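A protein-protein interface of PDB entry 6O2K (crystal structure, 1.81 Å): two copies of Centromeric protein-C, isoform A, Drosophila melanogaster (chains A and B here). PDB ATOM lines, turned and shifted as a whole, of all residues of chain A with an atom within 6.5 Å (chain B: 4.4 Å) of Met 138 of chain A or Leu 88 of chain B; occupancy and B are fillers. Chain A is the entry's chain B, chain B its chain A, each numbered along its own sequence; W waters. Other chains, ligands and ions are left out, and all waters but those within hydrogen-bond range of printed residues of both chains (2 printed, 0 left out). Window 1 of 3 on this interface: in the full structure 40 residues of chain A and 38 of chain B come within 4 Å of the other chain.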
ATOM      1  N   TYR A  56     -11.895 -20.053 -26.112  1.00  0.00           N
ATOM      2  CA  TYR A  56     -12.187 -20.830 -24.920  1.00  0.00           C
ATOM      3  C   TYR A  56     -13.166 -20.071 -24.037  1.00  0.00           C
ATOM      4  O   TYR A  56     -13.047 -18.855 -23.843  1.00  0.00           O
ATOM      5  CB  TYR A  56     -10.904 -21.131 -24.140  1.00  0.00           C
ATOM      6  CG  TYR A  56      -9.963 -22.081 -24.851  1.00  0.00           C
ATOM      7  CD1 TYR A  56     -10.144 -23.464 -24.766  1.00  0.00           C
ATOM      8  CD2 TYR A  56      -8.885 -21.603 -25.590  1.00  0.00           C
ATOM      9  CE1 TYR A  56      -9.280 -24.337 -25.407  1.00  0.00           C
ATOM     10  CE2 TYR A  56      -8.014 -22.472 -26.226  1.00  0.00           C
ATOM     11  CZ  TYR A  56      -8.223 -23.837 -26.135  1.00  0.00           C
ATOM     12  OH  TYR A  56      -7.360 -24.705 -26.773  1.00  0.00           O
ATOM     13  N   LEU A  64      -8.485 -15.999 -24.729  1.00  0.00           N
ATOM     14  CA  LEU A  64      -7.613 -17.010 -25.315  1.00  0.00           C
ATOM     15  C   LEU A  64      -8.408 -17.762 -26.376  1.00  0.00           C
ATOM     16  O   LEU A  64      -9.453 -18.335 -26.062  1.00  0.00           O
ATOM     17  CB  LEU A  64      -7.096 -17.966 -24.239  1.00  0.00           C
ATOM     18  CG  LEU A  64      -6.127 -19.045 -24.697  1.00  0.00           C
ATOM     19  CD1 LEU A  64      -4.836 -18.414 -25.118  1.00  0.00           C
ATOM     20  CD2 LEU A  64      -5.884 -20.047 -23.563  1.00  0.00           C
ATOM     21  N   GLY A  65      -7.947 -17.730 -27.624  1.00  0.00           N
ATOM     22  CA  GLY A  65      -8.729 -18.339 -28.685  1.00  0.00           C
ATOM     23  C   GLY A  65      -7.908 -18.562 -29.937  1.00  0.00           C
ATOM     24  O   GLY A  65      -6.685 -18.434 -29.931  1.00  0.00           O
ATOM     25  N   TYR A  66      -8.603 -18.885 -31.026  1.00  0.00           N
ATOM     26  CA  TYR A  66      -7.978 -19.185 -32.307  1.00  0.00           C
ATOM     27  C   TYR A  66      -8.632 -18.371 -33.407  1.00  0.00           C
ATOM     28  O   TYR A  66      -9.855 -18.167 -33.405  1.00  0.00           O
ATOM     29  CB  TYR A  66      -8.087 -20.683 -32.666  1.00  0.00           C
ATOM     30  CG  TYR A  66      -7.433 -21.582 -31.642  1.00  0.00           C
ATOM     31  CD1 TYR A  66      -6.070 -21.816 -31.667  1.00  0.00           C
ATOM     32  CD2 TYR A  66      -8.193 -22.187 -30.640  1.00  0.00           C
ATOM     33  CE1 TYR A  66      -5.462 -22.635 -30.703  1.00  0.00           C
ATOM     34  CE2 TYR A  66      -7.612 -23.005 -29.695  1.00  0.00           C
ATOM     35  CZ  TYR A  66      -6.245 -23.221 -29.725  1.00  0.00           C
ATOM     36  OH  TYR A  66      -5.685 -24.029 -28.758  1.00  0.00           O
ATOM     37  N   MET A  67      -7.804 -17.925 -34.351  1.00  0.00           N
ATOM     38  CA  MET A  67      -8.243 -17.366 -35.621  1.00  0.00           C
ATOM     39  C   MET A  67      -7.865 -18.333 -36.733  1.00  0.00           C
ATOM     40  O   MET A  67      -6.696 -18.723 -36.844  1.00  0.00           O
ATOM     41  CB  MET A  67      -7.592 -16.009 -35.879  1.00  0.00           C
ATOM     42  CG  MET A  67      -7.799 -14.991 -34.796  1.00  0.00           C
ATOM     43  SD  MET A  67      -7.113 -13.413 -35.358  1.00  0.00           S
ATOM     44  CE  MET A  67      -6.949 -12.521 -33.806  1.00  0.00           C
ATOM     45  N   LYS A  86      -0.953 -11.341 -27.752  1.00  0.00           N
ATOM     46  CA  LYS A  86       0.129 -12.094 -28.361  1.00  0.00           C
ATOM     47  C   LYS A  86      -0.482 -12.980 -29.440  1.00  0.00           C
ATOM     48  O   LYS A  86      -1.510 -13.619 -29.207  1.00  0.00           O
ATOM     49  CB  LYS A  86       0.866 -12.950 -27.323  1.00  0.00           C
ATOM     50  CG  LYS A  86       1.469 -12.141 -26.183  1.00  0.00           C
ATOM     51  CD  LYS A  86       2.271 -12.972 -25.207  1.00  0.00           C
ATOM     52  CE  LYS A  86       2.734 -12.092 -24.029  1.00  0.00           C
ATOM     53  NZ  LYS A  86       1.602 -11.563 -23.223  1.00  0.00           N
ATOM     54  N   LEU A  87       0.134 -13.000 -30.612  1.00  0.00           N
ATOM     55  CA  LEU A  87      -0.284 -13.875 -31.702  1.00  0.00           C
ATOM     56  C   LEU A  87       0.753 -14.980 -31.856  1.00  0.00           C
ATOM     57  O   LEU A  87       1.935 -14.702 -32.097  1.00  0.00           O
ATOM     58  CB  LEU A  87      -0.443 -13.082 -33.000  1.00  0.00           C
ATOM     59  CG  LEU A  87      -1.405 -11.880 -32.965  1.00  0.00           C
ATOM     60  CD1 LEU A  87      -1.341 -11.103 -34.276  1.00  0.00           C
ATOM     61  CD2 LEU A  87      -2.842 -12.339 -32.703  1.00  0.00           C
ATOM     62  N   LEU A  88       0.310 -16.227 -31.721  1.00  0.00           N
ATOM     63  CA  LEU A  88       1.193 -17.388 -31.723  1.00  0.00           C
ATOM     64  C   LEU A  88       0.716 -18.364 -32.789  1.00  0.00           C
ATOM     65  O   LEU A  88      -0.397 -18.899 -32.687  1.00  0.00           O
ATOM     66  CB  LEU A  88       1.209 -18.047 -30.341  1.00  0.00           C
ATOM     67  CG  LEU A  88       1.988 -19.344 -30.153  1.00  0.00           C
ATOM     68  CD1 LEU A  88       3.464 -19.140 -30.449  1.00  0.00           C
ATOM     69  CD2 LEU A  88       1.792 -19.822 -28.722  1.00  0.00           C
ATOM     70  N   VAL A  89       1.557 -18.617 -33.790  1.00  0.00           N
ATOM     71  CA  VAL A  89       1.135 -19.408 -34.944  1.00  0.00           C
ATOM     72  C   VAL A  89       1.005 -20.879 -34.551  1.00  0.00           C
ATOM     73  O   VAL A  89       1.948 -21.495 -34.035  1.00  0.00           O
ATOM     74  CB  VAL A  89       2.102 -19.219 -36.119  1.00  0.00           C
ATOM     75  CG1 VAL A  89       1.709 -20.110 -37.280  1.00  0.00           C
ATOM     76  CG2 VAL A  89       2.091 -17.752 -36.559  1.00  0.00           C
ATOM     77  N   GLN A  90      -0.180 -21.444 -34.793  1.00  0.00           N
ATOM     78  CA  GLN A  90      -0.470 -22.854 -34.546  1.00  0.00           C
ATOM     79  C   GLN A  90      -0.276 -23.708 -35.778  1.00  0.00           C
ATOM     80  O   GLN A  90       0.088 -24.892 -35.660  1.00  0.00           O
ATOM     81  CB  GLN A  90      -1.910 -23.023 -34.059  1.00  0.00           C
ATOM     82  CG  GLN A  90      -2.191 -22.291 -32.773  1.00  0.00           C
ATOM     83  CD  GLN A  90      -1.468 -22.942 -31.622  1.00  0.00           C
ATOM     84  OE1 GLN A  90      -1.715 -24.102 -31.304  1.00  0.00           O
ATOM     85  NE2 GLN A  90      -0.557 -22.200 -30.999  1.00  0.00           N
ATOM     86  N   VAL A 136      -3.673 -21.100 -39.051  1.00  0.00           N
ATOM     87  CA  VAL A 136      -4.329 -20.951 -37.759  1.00  0.00           C
ATOM     88  C   VAL A 136      -3.371 -20.268 -36.797  1.00  0.00           C
ATOM     89  O   VAL A 136      -2.214 -20.686 -36.673  1.00  0.00           O
ATOM     90  CB  VAL A 136      -4.756 -22.313 -37.183  1.00  0.00           C
ATOM     91  CG1 VAL A 136      -5.409 -22.136 -35.826  1.00  0.00           C
ATOM     92  CG2 VAL A 136      -5.686 -23.036 -38.146  1.00  0.00           C
ATOM     93  N   LEU A 137      -3.853 -19.241 -36.096  1.00  0.00           N
ATOM     94  CA  LEU A 137      -3.052 -18.648 -35.031  1.00  0.00           C
ATOM     95  C   LEU A 137      -3.838 -18.607 -33.734  1.00  0.00           C
ATOM     96  O   LEU A 137      -5.070 -18.558 -33.729  1.00  0.00           O
ATOM     97  CB  LEU A 137      -2.535 -17.239 -35.378  1.00  0.00           C
ATOM     98  CG  LEU A 137      -3.462 -16.039 -35.574  1.00  0.00           C
ATOM     99  CD1 LEU A 137      -3.962 -15.487 -34.253  1.00  0.00           C
ATOM    100  CD2 LEU A 137      -2.714 -14.958 -36.337  1.00  0.00           C
ATOM    101  N   MET A 138      -3.103 -18.664 -32.630  1.00  0.00           N
ATOM    102  CA  MET A 138      -3.675 -18.516 -31.299  1.00  0.00           C
ATOM    103  C   MET A 138      -3.573 -17.052 -30.899  1.00  0.00           C
ATOM    104  O   MET A 138      -2.525 -16.424 -31.076  1.00  0.00           O
ATOM    105  CB  MET A 138      -2.939 -19.401 -30.286  1.00  0.00           C
ATOM    106  CG  MET A 138      -3.484 -19.335 -28.851  1.00  0.00           C
ATOM    107  SD  MET A 138      -2.441 -20.273 -27.661  1.00  0.00           S
ATOM    108  CE  MET A 138      -2.829 -21.982 -28.094  1.00  0.00           C
ATOM    109  N   CYS A 139      -4.669 -16.515 -30.382  1.00  0.00           N
ATOM    110  CA  CYS A 139      -4.775 -15.134 -29.930  1.00  0.00           C
ATOM    111  C   CYS A 139      -4.846 -15.129 -28.406  1.00  0.00           C
ATOM    112  O   CYS A 139      -5.803 -15.674 -27.841  1.00  0.00           O
ATOM    113  CB  CYS A 139      -6.025 -14.502 -30.548  1.00  0.00           C
ATOM    114  SG  CYS A 139      -6.425 -12.844 -29.997  1.00  0.00           S
ATOM    115  N   ILE A 140      -3.852 -14.523 -27.756  1.00  0.00           N
ATOM    116  CA  ILE A 140      -3.727 -14.481 -26.306  1.00  0.00           C
ATOM    117  C   ILE A 140      -3.790 -13.022 -25.889  1.00  0.00           C
ATOM    118  O   ILE A 140      -2.852 -12.269 -26.156  1.00  0.00           O
ATOM    119  CB  ILE A 140      -2.407 -15.096 -25.831  1.00  0.00           C
ATOM    120  CG1 ILE A 140      -2.248 -16.515 -26.380  1.00  0.00           C
ATOM    121  CG2 ILE A 140      -2.315 -14.997 -24.306  1.00  0.00           C
ATOM    122  CD1 ILE A 140      -0.832 -17.125 -26.163  1.00  0.00           C
ATOM    123  N   LYS B  86      -2.912 -19.507 -16.814  1.00  0.00           N
ATOM    124  CA  LYS B  86      -3.631 -20.470 -17.640  1.00  0.00           C
ATOM    125  C   LYS B  86      -2.666 -21.569 -18.051  1.00  0.00           C
ATOM    126  O   LYS B  86      -1.530 -21.276 -18.445  1.00  0.00           O
ATOM    127  CB  LYS B  86      -4.240 -19.801 -18.872  1.00  0.00           C
ATOM    128  CG  LYS B  86      -5.388 -18.837 -18.579  1.00  0.00           C
ATOM    129  CD  LYS B  86      -5.803 -18.110 -19.865  1.00  0.00           C
ATOM    130  CE  LYS B  86      -6.961 -17.156 -19.648  1.00  0.00           C
ATOM    131  NZ  LYS B  86      -6.557 -15.908 -18.948  1.00  0.00           N
ATOM    132  N   LEU B  87      -3.106 -22.831 -17.950  1.00  0.00           N
ATOM    133  CA  LEU B  87      -2.311 -23.961 -18.413  1.00  0.00           C
ATOM    134  C   LEU B  87      -3.038 -24.647 -19.553  1.00  0.00           C
ATOM    135  O   LEU B  87      -4.188 -25.061 -19.391  1.00  0.00           O
ATOM    136  CB  LEU B  87      -2.029 -24.969 -17.282  1.00  0.00           C
ATOM    137  CG  LEU B  87      -1.392 -24.374 -16.012  1.00  0.00           C
ATOM    138  CD1 LEU B  87      -1.418 -25.390 -14.851  1.00  0.00           C
ATOM    139  CD2 LEU B  87       0.037 -23.899 -16.288  1.00  0.00           C
ATOM    140  N   LEU B  88      -2.358 -24.790 -20.693  1.00  0.00           N
ATOM    141  CA  LEU B  88      -2.961 -25.329 -21.911  1.00  0.00           C
ATOM    142  C   LEU B  88      -2.108 -26.474 -22.444  1.00  0.00           C
ATOM    143  O   LEU B  88      -0.918 -26.287 -22.709  1.00  0.00           O
ATOM    144  CB  LEU B  88      -3.103 -24.226 -22.975  1.00  0.00           C
ATOM    145  CG  LEU B  88      -3.776 -24.560 -24.314  1.00  0.00           C
ATOM    146  CD1 LEU B  88      -4.511 -23.360 -24.856  1.00  0.00           C
ATOM    147  CD2 LEU B  88      -2.738 -25.036 -25.326  1.00  0.00           C
ATOM    148  N   VAL B  89      -2.717 -27.643 -22.641  1.00  0.00           N
ATOM    149  CA  VAL B  89      -1.937 -28.820 -23.019  1.00  0.00           C
ATOM    150  C   VAL B  89      -1.487 -28.693 -24.468  1.00  0.00           C
ATOM    151  O   VAL B  89      -2.308 -28.622 -25.392  1.00  0.00           O
ATOM    152  CB  VAL B  89      -2.729 -30.116 -22.790  1.00  0.00           C
ATOM    153  CG1 VAL B  89      -1.882 -31.346 -23.170  1.00  0.00           C
ATOM    154  CG2 VAL B  89      -3.179 -30.202 -21.340  1.00  0.00           C
ATOM    155  N   GLN B  90      -0.173 -28.679 -24.668  1.00  0.00           N
ATOM    156  CA  GLN B  90       0.412 -28.658 -25.996  1.00  0.00           C
ATOM    157  C   GLN B  90       0.632 -30.058 -26.561  1.00  0.00           C
ATOM    158  O   GLN B  90       0.538 -30.251 -27.785  1.00  0.00           O
ATOM    159  CB  GLN B  90       1.740 -27.896 -25.958  1.00  0.00           C
ATOM    160  CG  GLN B  90       2.458 -27.881 -27.285  1.00  0.00           C
ATOM    161  CD  GLN B  90       1.782 -26.932 -28.246  1.00  0.00           C
ATOM    162  OE1 GLN B  90       1.447 -27.287 -29.373  1.00  0.00           O
ATOM    163  NE2 GLN B  90       1.547 -25.732 -27.791  1.00  0.00           N
ATOM    164  N   ASP B 115      -6.850 -28.836 -24.258  1.00  0.00           N
ATOM    165  CA  ASP B 115      -7.615 -28.436 -23.084  1.00  0.00           C
ATOM    166  C   ASP B 115      -6.822 -27.441 -22.249  1.00  0.00           C
ATOM    167  O   ASP B 115      -5.584 -27.451 -22.234  1.00  0.00           O
ATOM    168  CB  ASP B 115      -7.984 -29.654 -22.221  1.00  0.00           C
ATOM    169  CG  ASP B 115      -8.811 -30.678 -22.975  1.00  0.00           C
ATOM    170  OD1 ASP B 115      -9.420 -30.322 -24.005  1.00  0.00           O
ATOM    171  OD2 ASP B 115      -8.847 -31.857 -22.560  1.00  0.00           O
ATOM    172  N   MET B 116      -7.541 -26.579 -21.533  1.00  0.00           N
ATOM    173  CA  MET B 116      -6.887 -25.620 -20.652  1.00  0.00           C
ATOM    174  C   MET B 116      -7.619 -25.555 -19.321  1.00  0.00           C
ATOM    175  O   MET B 116      -8.766 -26.000 -19.181  1.00  0.00           O
ATOM    176  CB  MET B 116      -6.821 -24.201 -21.260  1.00  0.00           C
ATOM    177  CG  MET B 116      -8.191 -23.609 -21.519  1.00  0.00           C
ATOM    178  SD  MET B 116      -8.161 -21.823 -21.425  1.00  0.00           S
ATOM    179  CE  MET B 116      -7.694 -21.620 -19.704  1.00  0.00           C
ATOM    180  N   LEU B 137       3.162 -28.765 -21.578  1.00  0.00           N
ATOM    181  CA  LEU B 137       2.125 -27.844 -21.133  1.00  0.00           C
ATOM    182  C   LEU B 137       2.523 -26.427 -21.535  1.00  0.00           C
ATOM    183  O   LEU B 137       3.680 -26.036 -21.352  1.00  0.00           O
ATOM    184  CB  LEU B 137       1.981 -27.951 -19.610  1.00  0.00           C
ATOM    185  CG  LEU B 137       0.732 -27.523 -18.846  1.00  0.00           C
ATOM    186  CD1 LEU B 137      -0.475 -28.286 -19.358  1.00  0.00           C
ATOM    187  CD2 LEU B 137       0.948 -27.774 -17.354  1.00  0.00           C
ATOM    188  N   MET B 138       1.586 -25.657 -22.083  1.00  0.00           N
ATOM    189  CA  MET B 138       1.838 -24.232 -22.286  1.00  0.00           C
ATOM    190  C   MET B 138       1.398 -23.470 -21.046  1.00  0.00           C
ATOM    191  O   MET B 138       0.312 -23.710 -20.517  1.00  0.00           O
ATOM    192  CB  MET B 138       1.084 -23.697 -23.512  1.00  0.00           C
ATOM    193  CG  MET B 138       1.356 -22.212 -23.781  1.00  0.00           C
ATOM    194  SD  MET B 138       0.321 -21.569 -25.108  1.00  0.00           S
ATOM    195  CE  MET B 138       1.056 -22.387 -26.520  1.00  0.00           C
HETATM  196  O   HOH W   1      -0.032 -26.599 -31.195  1.00  0.00           O
HETATM  197  O   HOH W   2       2.144 -23.520 -29.634  1.00  0.00           O
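O of Leu 64 of chain A is in hydrogen-bond range of N of Tyr 56 of chain A.
OH of Tyr 66 of chain A sits at hydrogen-bond distance from OH of Tyr 56 of chain A (2.7 Å).
N of Met 138 of chain B sits at hydrogen-bond distance from O of Leu 88 of chain B (2.7 Å).
N of Met 138 of chain A sits at hydrogen-bond distance from O of Leu 88 of chain A (2.7 Å).
Tyr 56 of chain A touches Leu 88 of chain B.
CG of Met 116 of chain B touches CD1 of Tyr 56 of chain A, 3.8 Å away.
CD2 of Leu 64 of chain A touches CD1 of Leu 88 of chain B (3.8 Å).
Leu 64 of chain A touches Met 116 of chain B (CD2 to SD, 3.6 Å).
CD2 of Leu 88 of chain A touches CE of Met 138 of chain B, at 3.5 Å.
Met 138 of chain A touches Leu 88 of chain B.
Met 138 of chain A touches Met 138 of chain B (SD to SD, 3.98 Å).
Met 138 of chain A touches just these residues of chain B: Leu 88 and Met 138.
Leu 88 of chain B touches just these residues of chain A: Tyr 56 (3.7 Å), Leu 64 (3.8 Å) and Met 138 (3.9 Å).
Printed residues of chain B within 4 Å of Leu 88 of chain A: Met 138.
Of the printed residues of chain B, Tyr 56 of chain A touches Leu 88 and Met 116.
Printed residues of chain A within 4 Å of Met 138 of chain B: Leu 88 and Met 138.
Printed residues of chain B within 4 Å of Leu 64 of chain A: Leu 88 (3.8 Å) and Met 116 (3.6 Å).
Val 89 of chain B touches none of the printed residues of chain A.
The nearest printed residue of chain B that does not touch Leu 88 of chain A is Gln 90 of chain B (6.0 Å).
Of the 9 printed residues of chain B, 3 touch a printed residue of chain A.
Hydrophobic or aromatic side chains of chain A within 4 Å of the printed part of chain B: Tyr 56, Leu 64, Leu 88 and Met 138.
Among the printed residues, 7 pairs touch across the chains.
Among the printed residues, no Asp or Glu carboxylate lies within 4 Å of a Lys or Arg side-chain nitrogen of the other chain.
Leu 88 of chain A touches Met 138 of chain B, and with the chains exchanged Met 138 of chain A touches Leu 88 of chain B.
Met 138 of chain B touches its own counterpart, Met 138 of chain A.
Water W1 bridges OE1 of Gln 90 of chain B (2.4 Å) and OE1 of Gln 90 of chain A (3.0 Å).
Water W2 bridges NE2 of Gln 90 of chain B (2.9 Å) and NE2 of Gln 90 of chain A (3.3 Å).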
